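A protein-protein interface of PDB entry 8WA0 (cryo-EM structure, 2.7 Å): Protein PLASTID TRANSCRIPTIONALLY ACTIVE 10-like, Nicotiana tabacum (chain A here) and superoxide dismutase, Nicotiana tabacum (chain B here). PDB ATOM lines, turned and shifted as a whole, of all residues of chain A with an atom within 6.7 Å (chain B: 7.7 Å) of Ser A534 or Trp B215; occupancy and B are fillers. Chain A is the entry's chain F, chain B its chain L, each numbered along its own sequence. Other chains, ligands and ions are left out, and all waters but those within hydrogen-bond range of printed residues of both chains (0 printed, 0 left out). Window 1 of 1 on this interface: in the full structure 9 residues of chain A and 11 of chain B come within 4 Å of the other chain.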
ATOM      1  N   GLU A 527     -10.297  16.512 -33.618  1.00  0.00           N
ATOM      2  CA  GLU A 527     -10.059  15.120 -33.463  1.00  0.00           C
ATOM      3  C   GLU A 527     -10.080  14.788 -32.012  1.00  0.00           C
ATOM      4  O   GLU A 527     -10.632  13.774 -31.600  1.00  0.00           O
ATOM      5  CB  GLU A 527      -8.725  14.758 -34.130  1.00  0.00           C
ATOM      6  N   MET A 529     -11.580  16.395 -29.779  1.00  0.00           N
ATOM      7  CA  MET A 529     -12.864  16.585 -29.241  1.00  0.00           C
ATOM      8  C   MET A 529     -13.565  15.310 -29.413  1.00  0.00           C
ATOM      9  O   MET A 529     -14.281  14.884 -28.532  1.00  0.00           O
ATOM     10  CB  MET A 529     -13.577  17.652 -30.042  1.00  0.00           C
ATOM     11  CG  MET A 529     -14.947  18.041 -29.516  1.00  0.00           C
ATOM     12  SD  MET A 529     -15.826  19.108 -30.674  1.00  0.00           S
ATOM     13  CE  MET A 529     -14.595  20.377 -30.964  1.00  0.00           C
ATOM     14  N   LEU A 530     -13.381  14.673 -30.546  1.00  0.00           N
ATOM     15  CA  LEU A 530     -14.136  13.476 -30.815  1.00  0.00           C
ATOM     16  C   LEU A 530     -13.755  12.455 -29.835  1.00  0.00           C
ATOM     17  O   LEU A 530     -14.582  11.715 -29.333  1.00  0.00           O
ATOM     18  CB  LEU A 530     -13.928  13.003 -32.229  1.00  0.00           C
ATOM     19  CG  LEU A 530     -14.526  13.912 -33.299  1.00  0.00           C
ATOM     20  CD1 LEU A 530     -14.118  13.457 -34.690  1.00  0.00           C
ATOM     21  CD2 LEU A 530     -16.037  13.974 -33.162  1.00  0.00           C
ATOM     22  N   ARG A 531     -12.491  12.435 -29.530  1.00  0.00           N
ATOM     23  CA  ARG A 531     -12.021  11.500 -28.570  1.00  0.00           C
ATOM     24  C   ARG A 531     -12.644  11.757 -27.196  1.00  0.00           C
ATOM     25  O   ARG A 531     -13.037  10.825 -26.515  1.00  0.00           O
ATOM     26  CB  ARG A 531     -10.512  11.542 -28.581  1.00  0.00           C
ATOM     27  CG  ARG A 531      -9.816  10.421 -27.843  1.00  0.00           C
ATOM     28  CD  ARG A 531      -8.344  10.757 -27.792  1.00  0.00           C
ATOM     29  NE  ARG A 531      -7.956  11.477 -29.001  1.00  0.00           N
ATOM     30  CZ  ARG A 531      -6.794  12.094 -29.161  1.00  0.00           C
ATOM     31  NH1 ARG A 531      -5.899  12.080 -28.185  1.00  0.00           N
ATOM     32  NH2 ARG A 531      -6.527  12.726 -30.294  1.00  0.00           N
ATOM     33  N   ASP A 532     -12.755  13.010 -26.779  1.00  0.00           N
ATOM     34  CA  ASP A 532     -13.394  13.369 -25.515  1.00  0.00           C
ATOM     35  C   ASP A 532     -14.834  13.062 -25.454  1.00  0.00           C
ATOM     36  O   ASP A 532     -15.314  12.670 -24.425  1.00  0.00           O
ATOM     37  CB  ASP A 532     -13.338  14.869 -25.379  1.00  0.00           C
ATOM     38  CG  ASP A 532     -13.921  15.367 -24.081  1.00  0.00           C
ATOM     39  OD1 ASP A 532     -13.647  14.755 -23.034  1.00  0.00           O
ATOM     40  OD2 ASP A 532     -14.645  16.384 -24.107  1.00  0.00           O
ATOM     41  N   ILE A 533     -15.564  13.262 -26.534  1.00  0.00           N
ATOM     42  CA  ILE A 533     -16.986  13.122 -26.469  1.00  0.00           C
ATOM     43  C   ILE A 533     -17.186  11.773 -26.032  1.00  0.00           C
ATOM     44  O   ILE A 533     -17.985  11.497 -25.162  1.00  0.00           O
ATOM     45  CB  ILE A 533     -17.631  13.229 -27.827  1.00  0.00           C
ATOM     46  CG1 ILE A 533     -17.384  14.609 -28.429  1.00  0.00           C
ATOM     47  CG2 ILE A 533     -19.126  12.990 -27.728  1.00  0.00           C
ATOM     48  CD1 ILE A 533     -17.957  15.746 -27.615  1.00  0.00           C
ATOM     49  N   SER A 534     -16.467  10.852 -26.648  1.00  0.00           N
ATOM     50  CA  SER A 534     -16.689   9.454 -26.346  1.00  0.00           C
ATOM     51  C   SER A 534     -16.199   9.098 -24.973  1.00  0.00           C
ATOM     52  O   SER A 534     -16.842   8.335 -24.256  1.00  0.00           O
ATOM     53  CB  SER A 534     -16.009   8.587 -27.391  1.00  0.00           C
ATOM     54  OG  SER A 534     -14.727   9.093 -27.696  1.00  0.00           O
ATOM     55  N   CYS A 535     -15.062   9.657 -24.593  1.00  0.00           N
ATOM     56  CA  CYS A 535     -14.505   9.331 -23.302  1.00  0.00           C
ATOM     57  C   CYS A 535     -15.472   9.763 -22.233  1.00  0.00           C
ATOM     58  O   CYS A 535     -15.741   9.022 -21.298  1.00  0.00           O
ATOM     59  CB  CYS A 535     -13.182  10.056 -23.102  1.00  0.00           C
ATOM     60  SG  CYS A 535     -11.763   9.273 -23.901  1.00  0.00           S
ATOM     61  N   ARG A 536     -16.033  10.950 -22.390  1.00  0.00           N
ATOM     62  CA  ARG A 536     -16.944  11.460 -21.392  1.00  0.00           C
ATOM     63  C   ARG A 536     -18.234  10.687 -21.420  1.00  0.00           C
ATOM     64  O   ARG A 536     -18.766  10.335 -20.371  1.00  0.00           O
ATOM     65  CB  ARG A 536     -17.208  12.944 -21.607  1.00  0.00           C
ATOM     66  CG  ARG A 536     -16.253  13.843 -20.839  1.00  0.00           C
ATOM     67  CD  ARG A 536     -16.646  15.307 -20.948  1.00  0.00           C
ATOM     68  NE  ARG A 536     -16.046  16.114 -19.888  1.00  0.00           N
ATOM     69  CZ  ARG A 536     -14.897  16.776 -20.001  1.00  0.00           C
ATOM     70  NH1 ARG A 536     -14.214  16.740 -21.131  1.00  0.00           N
ATOM     71  NH2 ARG A 536     -14.432  17.481 -18.983  1.00  0.00           N
ATOM     72  N   ARG A 537     -18.735  10.394 -22.612  1.00  0.00           N
ATOM     73  CA  ARG A 537     -19.999   9.718 -22.704  1.00  0.00           C
ATOM     74  C   ARG A 537     -20.042   8.379 -22.041  1.00  0.00           C
ATOM     75  O   ARG A 537     -21.108   7.891 -21.693  1.00  0.00           O
ATOM     76  CB  ARG A 537     -20.490   9.657 -24.117  1.00  0.00           C
ATOM     77  CG  ARG A 537     -21.211  10.910 -24.562  1.00  0.00           C
ATOM     78  CD  ARG A 537     -22.517  11.070 -23.809  1.00  0.00           C
ATOM     79  NE  ARG A 537     -23.383   9.908 -23.979  1.00  0.00           N
ATOM     80  CZ  ARG A 537     -24.596   9.799 -23.450  1.00  0.00           C
ATOM     81  NH1 ARG A 537     -25.091  10.786 -22.716  1.00  0.00           N
ATOM     82  NH2 ARG A 537     -25.316   8.705 -23.652  1.00  0.00           N
ATOM     83  N   ALA A 538     -18.885   7.757 -21.863  1.00  0.00           N
ATOM     84  CA  ALA A 538     -18.829   6.438 -21.251  1.00  0.00           C
ATOM     85  C   ALA A 538     -18.439   6.543 -19.799  1.00  0.00           C
ATOM     86  O   ALA A 538     -18.717   5.651 -19.002  1.00  0.00           O
ATOM     87  CB  ALA A 538     -17.839   5.565 -21.988  1.00  0.00           C
ATOM     88  N   LEU A 539     -17.795   7.644 -19.447  1.00  0.00           N
ATOM     89  CA  LEU A 539     -17.357   7.830 -18.077  1.00  0.00           C
ATOM     90  C   LEU A 539     -18.406   8.521 -17.219  1.00  0.00           C
ATOM     91  O   LEU A 539     -18.164   8.786 -16.048  1.00  0.00           O
ATOM     92  CB  LEU A 539     -16.041   8.596 -18.040  1.00  0.00           C
ATOM     93  CG  LEU A 539     -14.817   7.756 -18.388  1.00  0.00           C
ATOM     94  CD1 LEU A 539     -13.573   8.624 -18.460  1.00  0.00           C
ATOM     95  CD2 LEU A 539     -14.651   6.645 -17.365  1.00  0.00           C
ATOM     96  N   LEU A 543     -21.124  16.879 -20.233  1.00  0.00           N
ATOM     97  CA  LEU A 543     -20.850  17.336 -21.561  1.00  0.00           C
ATOM     98  C   LEU A 543     -20.647  18.809 -21.787  1.00  0.00           C
ATOM     99  O   LEU A 543     -19.734  19.202 -22.505  1.00  0.00           O
ATOM    100  CB  LEU A 543     -21.937  16.833 -22.468  1.00  0.00           C
ATOM    101  CG  LEU A 543     -21.942  15.321 -22.701  1.00  0.00           C
ATOM    102  CD1 LEU A 543     -23.119  14.926 -23.579  1.00  0.00           C
ATOM    103  CD2 LEU A 543     -20.631  14.867 -23.323  1.00  0.00           C
ATOM    104  N   LEU B 104     -20.340  -0.612 -34.405  1.00  0.00           N
ATOM    105  CA  LEU B 104     -20.468   0.710 -34.892  1.00  0.00           C
ATOM    106  C   LEU B 104     -21.901   1.142 -34.743  1.00  0.00           C
ATOM    107  O   LEU B 104     -22.176   2.270 -34.334  1.00  0.00           O
ATOM    108  CB  LEU B 104     -20.011   0.755 -36.333  1.00  0.00           C
ATOM    109  CG  LEU B 104     -19.764   2.140 -36.923  1.00  0.00           C
ATOM    110  CD1 LEU B 104     -18.737   2.890 -36.090  1.00  0.00           C
ATOM    111  CD2 LEU B 104     -19.303   2.021 -38.366  1.00  0.00           C
ATOM    112  N   ARG B 109     -23.078   6.830 -32.267  1.00  0.00           N
ATOM    113  CA  ARG B 109     -22.605   8.191 -32.218  1.00  0.00           C
ATOM    114  C   ARG B 109     -22.726   8.748 -30.829  1.00  0.00           C
ATOM    115  O   ARG B 109     -22.357   8.102 -29.865  1.00  0.00           O
ATOM    116  CB  ARG B 109     -23.341   9.070 -33.211  1.00  0.00           C
ATOM    117  N   GLY B 110     -23.340   9.907 -30.679  1.00  0.00           N
ATOM    118  CA  GLY B 110     -23.344  10.531 -29.368  1.00  0.00           C
ATOM    119  C   GLY B 110     -23.949   9.696 -28.257  1.00  0.00           C
ATOM    120  O   GLY B 110     -23.419   9.678 -27.149  1.00  0.00           O
ATOM    121  N   LEU B 112     -24.655   6.273 -26.655  1.00  0.00           N
ATOM    122  CA  LEU B 112     -24.419   4.860 -26.692  1.00  0.00           C
ATOM    123  C   LEU B 112     -25.763   4.166 -26.552  1.00  0.00           C
ATOM    124  O   LEU B 112     -26.523   4.464 -25.638  1.00  0.00           O
ATOM    125  CB  LEU B 112     -23.477   4.445 -25.564  1.00  0.00           C
ATOM    126  CG  LEU B 112     -21.988   4.797 -25.584  1.00  0.00           C
ATOM    127  CD1 LEU B 112     -21.727   6.281 -25.379  1.00  0.00           C
ATOM    128  CD2 LEU B 112     -21.279   3.997 -24.504  1.00  0.00           C
ATOM    129  N   TRP B 176      -4.387   0.992 -26.657  1.00  0.00           N
ATOM    130  CA  TRP B 176      -4.339   0.661 -28.084  1.00  0.00           C
ATOM    131  C   TRP B 176      -3.163   1.141 -28.913  1.00  0.00           C
ATOM    132  O   TRP B 176      -2.545   2.142 -28.577  1.00  0.00           O
ATOM    133  CB  TRP B 176      -5.604   1.175 -28.775  1.00  0.00           C
ATOM    134  CG  TRP B 176      -6.897   0.612 -28.277  1.00  0.00           C
ATOM    135  CD1 TRP B 176      -7.693   1.139 -27.311  1.00  0.00           C
ATOM    136  CD2 TRP B 176      -7.560  -0.568 -28.745  1.00  0.00           C
ATOM    137  NE1 TRP B 176      -8.804   0.354 -27.131  1.00  0.00           N
ATOM    138  CE2 TRP B 176      -8.748  -0.699 -28.004  1.00  0.00           C
ATOM    139  CE3 TRP B 176      -7.266  -1.523 -29.718  1.00  0.00           C
ATOM    140  CZ2 TRP B 176      -9.639  -1.750 -28.201  1.00  0.00           C
ATOM    141  CZ3 TRP B 176      -8.151  -2.565 -29.913  1.00  0.00           C
ATOM    142  CH2 TRP B 176      -9.322  -2.670 -29.158  1.00  0.00           C
ATOM    143  N   ALA B 178      -2.519   2.051 -32.961  1.00  0.00           N
ATOM    144  CA  ALA B 178      -3.436   2.213 -34.085  1.00  0.00           C
ATOM    145  C   ALA B 178      -2.925   2.979 -35.287  1.00  0.00           C
ATOM    146  O   ALA B 178      -1.847   3.564 -35.248  1.00  0.00           O
ATOM    147  CB  ALA B 178      -4.743   2.821 -33.601  1.00  0.00           C
ATOM    148  N   TYR B 179      -3.694   2.950 -36.369  1.00  0.00           N
ATOM    149  CA  TYR B 179      -3.303   3.656 -37.577  1.00  0.00           C
ATOM    150  C   TYR B 179      -4.174   4.853 -37.886  1.00  0.00           C
ATOM    151  O   TYR B 179      -5.347   4.862 -37.541  1.00  0.00           O
ATOM    152  CB  TYR B 179      -3.307   2.689 -38.754  1.00  0.00           C
ATOM    153  CG  TYR B 179      -2.717   3.253 -40.024  1.00  0.00           C
ATOM    154  CD1 TYR B 179      -1.379   3.620 -40.087  1.00  0.00           C
ATOM    155  CD2 TYR B 179      -3.495   3.414 -41.161  1.00  0.00           C
ATOM    156  CE1 TYR B 179      -0.836   4.137 -41.246  1.00  0.00           C
ATOM    157  CE2 TYR B 179      -2.960   3.929 -42.324  1.00  0.00           C
ATOM    158  CZ  TYR B 179      -1.631   4.288 -42.361  1.00  0.00           C
ATOM    159  OH  TYR B 179      -1.098   4.799 -43.522  1.00  0.00           O
ATOM    160  N   ALA B 181      -5.810   6.046 -40.478  1.00  0.00           N
ATOM    161  CA  ALA B 181      -6.623   6.183 -41.671  1.00  0.00           C
ATOM    162  C   ALA B 181      -7.885   6.791 -41.129  1.00  0.00           C
ATOM    163  O   ALA B 181      -8.784   6.067 -40.715  1.00  0.00           O
ATOM    164  CB  ALA B 181      -6.898   4.849 -42.331  1.00  0.00           C
ATOM    165  N   ASN B 182      -7.970   8.118 -41.131  1.00  0.00           N
ATOM    166  CA  ASN B 182      -9.120   8.768 -40.513  1.00  0.00           C
ATOM    167  C   ASN B 182      -9.970   9.620 -41.429  1.00  0.00           C
ATOM    168  O   ASN B 182      -9.476  10.480 -42.160  1.00  0.00           O
ATOM    169  CB  ASN B 182      -8.683   9.550 -39.287  1.00  0.00           C
ATOM    170  CG  ASN B 182      -7.633  10.603 -39.595  1.00  0.00           C
ATOM    171  OD1 ASN B 182      -6.774  10.419 -40.457  1.00  0.00           O
ATOM    172  ND2 ASN B 182      -7.693  11.717 -38.878  1.00  0.00           N
ATOM    173  N   ARG B 183     -11.265   9.389 -41.377  1.00  0.00           N
ATOM    174  CA  ARG B 183     -12.143  10.129 -42.253  1.00  0.00           C
ATOM    175  C   ARG B 183     -12.653  11.397 -41.592  1.00  0.00           C
ATOM    176  O   ARG B 183     -13.320  11.329 -40.560  1.00  0.00           O
ATOM    177  CB  ARG B 183     -13.333   9.259 -42.626  1.00  0.00           C
ATOM    178  N   VAL B 202      -0.451   5.663 -33.783  1.00  0.00           N
ATOM    179  CA  VAL B 202      -0.922   6.315 -32.574  1.00  0.00           C
ATOM    180  C   VAL B 202      -1.213   5.384 -31.418  1.00  0.00           C
ATOM    181  O   VAL B 202      -1.620   4.246 -31.618  1.00  0.00           O
ATOM    182  CB  VAL B 202      -2.166   7.172 -32.870  1.00  0.00           C
ATOM    183  CG1 VAL B 202      -1.775   8.443 -33.603  1.00  0.00           C
ATOM    184  CG2 VAL B 202      -3.191   6.384 -33.670  1.00  0.00           C
ATOM    185  N   VAL B 203      -0.986   5.860 -30.203  1.00  0.00           N
ATOM    186  CA  VAL B 203      -1.313   5.061 -29.032  1.00  0.00           C
ATOM    187  C   VAL B 203      -2.404   5.786 -28.256  1.00  0.00           C
ATOM    188  O   VAL B 203      -2.246   6.955 -27.915  1.00  0.00           O
ATOM    189  CB  VAL B 203      -0.073   4.835 -28.154  1.00  0.00           C
ATOM    190  CG1 VAL B 203      -0.452   4.190 -26.829  1.00  0.00           C
ATOM    191  CG2 VAL B 203       0.948   3.986 -28.893  1.00  0.00           C
ATOM    192  N   VAL B 204      -3.525   5.117 -27.998  1.00  0.00           N
ATOM    193  CA  VAL B 204      -4.631   5.745 -27.273  1.00  0.00           C
ATOM    194  C   VAL B 204      -5.097   4.964 -26.050  1.00  0.00           C
ATOM    195  O   VAL B 204      -4.770   3.785 -25.897  1.00  0.00           O
ATOM    196  CB  VAL B 204      -5.850   5.983 -28.182  1.00  0.00           C
ATOM    197  CG1 VAL B 204      -5.621   7.180 -29.094  1.00  0.00           C
ATOM    198  CG2 VAL B 204      -6.175   4.737 -28.986  1.00  0.00           C
ATOM    199  N   LYS B 205      -5.858   5.619 -25.176  1.00  0.00           N
ATOM    200  CA  LYS B 205      -6.389   4.949 -23.998  1.00  0.00           C
ATOM    201  C   LYS B 205      -7.895   4.956 -24.098  1.00  0.00           C
ATOM    202  O   LYS B 205      -8.493   5.987 -24.380  1.00  0.00           O
ATOM    203  CB  LYS B 205      -5.956   5.667 -22.729  1.00  0.00           C
ATOM    204  N   THR B 206      -8.515   3.808 -23.894  1.00  0.00           N
ATOM    205  CA  THR B 206      -9.949   3.729 -24.020  1.00  0.00           C
ATOM    206  C   THR B 206     -10.573   3.209 -22.745  1.00  0.00           C
ATOM    207  O   THR B 206     -10.162   2.182 -22.221  1.00  0.00           O
ATOM    208  CB  THR B 206     -10.337   2.814 -25.178  1.00  0.00           C
ATOM    209  N   PRO B 207     -11.574   3.922 -22.238  1.00  0.00           N
ATOM    210  CA  PRO B 207     -12.236   3.499 -21.008  1.00  0.00           C
ATOM    211  C   PRO B 207     -13.296   2.457 -21.235  1.00  0.00           C
ATOM    212  O   PRO B 207     -14.100   2.621 -22.146  1.00  0.00           O
ATOM    213  CB  PRO B 207     -12.906   4.780 -20.526  1.00  0.00           C
ATOM    214  CG  PRO B 207     -13.092   5.620 -21.742  1.00  0.00           C
ATOM    215  CD  PRO B 207     -11.954   5.284 -22.652  1.00  0.00           C
ATOM    216  N   ALA B 209     -15.712  -0.014 -22.533  1.00  0.00           N
ATOM    217  CA  ALA B 209     -15.953  -0.510 -23.889  1.00  0.00           C
ATOM    218  C   ALA B 209     -15.688   0.455 -25.043  1.00  0.00           C
ATOM    219  O   ALA B 209     -16.636   0.907 -25.679  1.00  0.00           O
ATOM    220  CB  ALA B 209     -17.380  -1.023 -23.993  1.00  0.00           C
ATOM    221  N   VAL B 210     -14.426   0.754 -25.343  1.00  0.00           N
ATOM    222  CA  VAL B 210     -14.130   1.601 -26.500  1.00  0.00           C
ATOM    223  C   VAL B 210     -13.104   1.021 -27.483  1.00  0.00           C
ATOM    224  O   VAL B 210     -12.027   0.606 -27.067  1.00  0.00           O
ATOM    225  CB  VAL B 210     -13.681   3.011 -26.064  1.00  0.00           C
ATOM    226  CG1 VAL B 210     -13.313   3.864 -27.272  1.00  0.00           C
ATOM    227  CG2 VAL B 210     -14.761   3.711 -25.253  1.00  0.00           C
ATOM    228  N   ASN B 211     -13.424   0.990 -28.781  1.00  0.00           N
ATOM    229  CA  ASN B 211     -12.472   0.531 -29.804  1.00  0.00           C
ATOM    230  C   ASN B 211     -12.212   1.674 -30.810  1.00  0.00           C
ATOM    231  O   ASN B 211     -13.162   2.325 -31.226  1.00  0.00           O
ATOM    232  CB  ASN B 211     -12.961  -0.724 -30.517  1.00  0.00           C
ATOM    233  CG  ASN B 211     -14.442  -0.689 -30.826  1.00  0.00           C
ATOM    234  OD1 ASN B 211     -14.899   0.075 -31.674  1.00  0.00           O
ATOM    235  ND2 ASN B 211     -15.201  -1.539 -30.147  1.00  0.00           N
ATOM    236  N   PRO B 212     -10.932   1.954 -31.181  1.00  0.00           N
ATOM    237  CA  PRO B 212     -10.739   3.107 -32.071  1.00  0.00           C
ATOM    238  C   PRO B 212     -11.627   3.141 -33.307  1.00  0.00           C
ATOM    239  O   PRO B 212     -11.748   4.215 -33.869  1.00  0.00           O
ATOM    240  CB  PRO B 212      -9.265   3.014 -32.434  1.00  0.00           C
ATOM    241  CG  PRO B 212      -8.643   2.387 -31.235  1.00  0.00           C
ATOM    242  CD  PRO B 212      -9.651   1.399 -30.720  1.00  0.00           C
ATOM    243  N   LEU B 213     -12.202   2.024 -33.738  1.00  0.00           N
ATOM    244  CA  LEU B 213     -13.161   2.027 -34.842  1.00  0.00           C
ATOM    245  C   LEU B 213     -14.261   3.066 -34.675  1.00  0.00           C
ATOM    246  O   LEU B 213     -14.715   3.646 -35.658  1.00  0.00           O
ATOM    247  CB  LEU B 213     -13.797   0.642 -34.936  1.00  0.00           C
ATOM    248  CG  LEU B 213     -14.908   0.400 -35.956  1.00  0.00           C
ATOM    249  CD1 LEU B 213     -14.310   0.149 -37.331  1.00  0.00           C
ATOM    250  CD2 LEU B 213     -15.763  -0.782 -35.525  1.00  0.00           C
ATOM    251  N   VAL B 214     -14.713   3.292 -33.447  1.00  0.00           N
ATOM    252  CA  VAL B 214     -15.741   4.265 -33.173  1.00  0.00           C
ATOM    253  C   VAL B 214     -15.265   5.579 -33.722  1.00  0.00           C
ATOM    254  O   VAL B 214     -16.024   6.295 -34.367  1.00  0.00           O
ATOM    255  CB  VAL B 214     -15.970   4.384 -31.674  1.00  0.00           C
ATOM    256  CG1 VAL B 214     -16.676   5.683 -31.320  1.00  0.00           C
ATOM    257  CG2 VAL B 214     -16.756   3.189 -31.162  1.00  0.00           C
ATOM    258  N   TRP B 215     -13.996   5.898 -33.535  1.00  0.00           N
ATOM    259  CA  TRP B 215     -13.477   7.104 -34.151  1.00  0.00           C
ATOM    260  C   TRP B 215     -12.651   6.796 -35.375  1.00  0.00           C
ATOM    261  O   TRP B 215     -11.894   7.643 -35.835  1.00  0.00           O
ATOM    262  CB  TRP B 215     -12.787   8.052 -33.164  1.00  0.00           C
ATOM    263  CG  TRP B 215     -11.645   7.528 -32.370  1.00  0.00           C
ATOM    264  CD1 TRP B 215     -10.425   7.148 -32.834  1.00  0.00           C
ATOM    265  CD2 TRP B 215     -11.591   7.404 -30.947  1.00  0.00           C
ATOM    266  NE1 TRP B 215      -9.621   6.761 -31.790  1.00  0.00           N
ATOM    267  CE2 TRP B 215     -10.315   6.911 -30.618  1.00  0.00           C
ATOM    268  CE3 TRP B 215     -12.504   7.647 -29.919  1.00  0.00           C
ATOM    269  CZ2 TRP B 215      -9.930   6.654 -29.307  1.00  0.00           C
ATOM    270  CZ3 TRP B 215     -12.120   7.391 -28.621  1.00  0.00           C
ATOM    271  CH2 TRP B 215     -10.844   6.897 -28.326  1.00  0.00           C
ATOM    272  N   ASP B 216     -12.771   5.579 -35.891  1.00  0.00           N
ATOM    273  CA  ASP B 216     -12.077   5.185 -37.115  1.00  0.00           C
ATOM    274  C   ASP B 216     -10.579   5.318 -37.192  1.00  0.00           C
ATOM    275  O   ASP B 216     -10.059   5.772 -38.198  1.00  0.00           O
ATOM    276  CB  ASP B 216     -12.725   5.807 -38.347  1.00  0.00           C
ATOM    277  CG  ASP B 216     -13.762   4.903 -38.970  1.00  0.00           C
ATOM    278  OD1 ASP B 216     -13.856   3.734 -38.543  1.00  0.00           O
ATOM    279  OD2 ASP B 216     -14.475   5.355 -39.890  1.00  0.00           O
ATOM    280  N   TYR B 217      -9.868   4.953 -36.141  1.00  0.00           N
ATOM    281  CA  TYR B 217      -8.417   4.914 -36.254  1.00  0.00           C
ATOM    282  C   TYR B 217      -8.217   3.409 -36.345  1.00  0.00           C
ATOM    283  O   TYR B 217      -8.749   2.680 -35.513  1.00  0.00           O
ATOM    284  CB  TYR B 217      -7.725   5.469 -35.016  1.00  0.00           C
ATOM    285  CG  TYR B 217      -7.651   6.975 -34.931  1.00  0.00           C
ATOM    286  CD1 TYR B 217      -8.330   7.781 -35.830  1.00  0.00           C
ATOM    287  CD2 TYR B 217      -6.904   7.587 -33.937  1.00  0.00           C
ATOM    288  CE1 TYR B 217      -8.269   9.157 -35.739  1.00  0.00           C
ATOM    289  CE2 TYR B 217      -6.836   8.961 -33.837  1.00  0.00           C
ATOM    290  CZ  TYR B 217      -7.519   9.742 -34.743  1.00  0.00           C
ATOM    291  OH  TYR B 217      -7.453  11.113 -34.656  1.00  0.00           O
ATOM    292  N   SER B 218      -7.439   2.913 -37.306  1.00  0.00           N
ATOM    293  CA  SER B 218      -7.306   1.458 -37.487  1.00  0.00           C
ATOM    294  C   SER B 218      -6.520   0.724 -36.402  1.00  0.00           C
ATOM    295  O   SER B 218      -5.306   0.836 -36.345  1.00  0.00           O
ATOM    296  CB  SER B 218      -6.703   1.165 -38.851  1.00  0.00           C
ATOM    297  OG  SER B 218      -7.450   1.803 -39.870  1.00  0.00           O
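Of the printed residues of chain B, Glu A527 touches Tyr B217 (3.9 Å).
Ser A534 touches just one residue of chain B: Trp B215.
Printed residues of chain B within 4 Å of Arg A537: Gly B110 and Leu B112.
Printed residues of chain A within 4 Å of Leu B112: Arg A537.
Trp B215 touches just these residues of chain A: Arg A531 and Ser A534.
Of the printed residues of chain A, Tyr B217 touches Glu A527.
The nearest residue of chain A that does not touch Trp B215 is Leu A530 (4.6 Å).
The nearest printed residue of chain A that does not touch Gly B110 is Ile A533 (5.2 Å).
Glu A527 touches Tyr B217 (CB to OH, 3.9 Å).
CH2 of Trp B215 touches CG of Arg A531 (3.7 Å).
Ser A534 touches Trp B215 (OG to CZ3, 3.2 Å).
CB of Arg A537 touches CD1 of Leu B112, 3.8 Å away.
The backbone carbonyl oxygen (O) of Gly B110 lies within hydrogen-bond range of the guanidinium group (NE) of Arg A537 (3.2 Å).
O of Pro B212 lies within hydrogen-bond range of N of Tyr B217 (3.0 Å).
The backbone carbonyl oxygen of Leu A530 sits at hydrogen-bond distance from the side-chain hydroxyl of Ser A534 (3.1 Å).
O of Arg A531 is in hydrogen-bond range of OG of Ser A534 (2.7 Å).
The backbone carbonyl oxygen (O) of Arg A531 lies within hydrogen-bond range of the side-chain sulfur (SG) of Cys A535, at 3.3 Å.
Of the 13 printed residues of chain A, 4 touch a printed residue of chain B.
Printed residues of chain A that touch a printed residue of chain B: Glu A527, Arg A531, Ser A534 and Arg A537.
Of the 26 printed residues of chain B, 4 touch a printed residue of chain A.
Along chain B the printed residues that touch a printed residue of chain A span positions 110 to 217.
Among the printed residues, 5 pairs touch across the chains.
Among the printed residues, no Asp or Glu carboxylate lies within 4 Å of a Lys or Arg side-chain nitrogen of the other chain.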
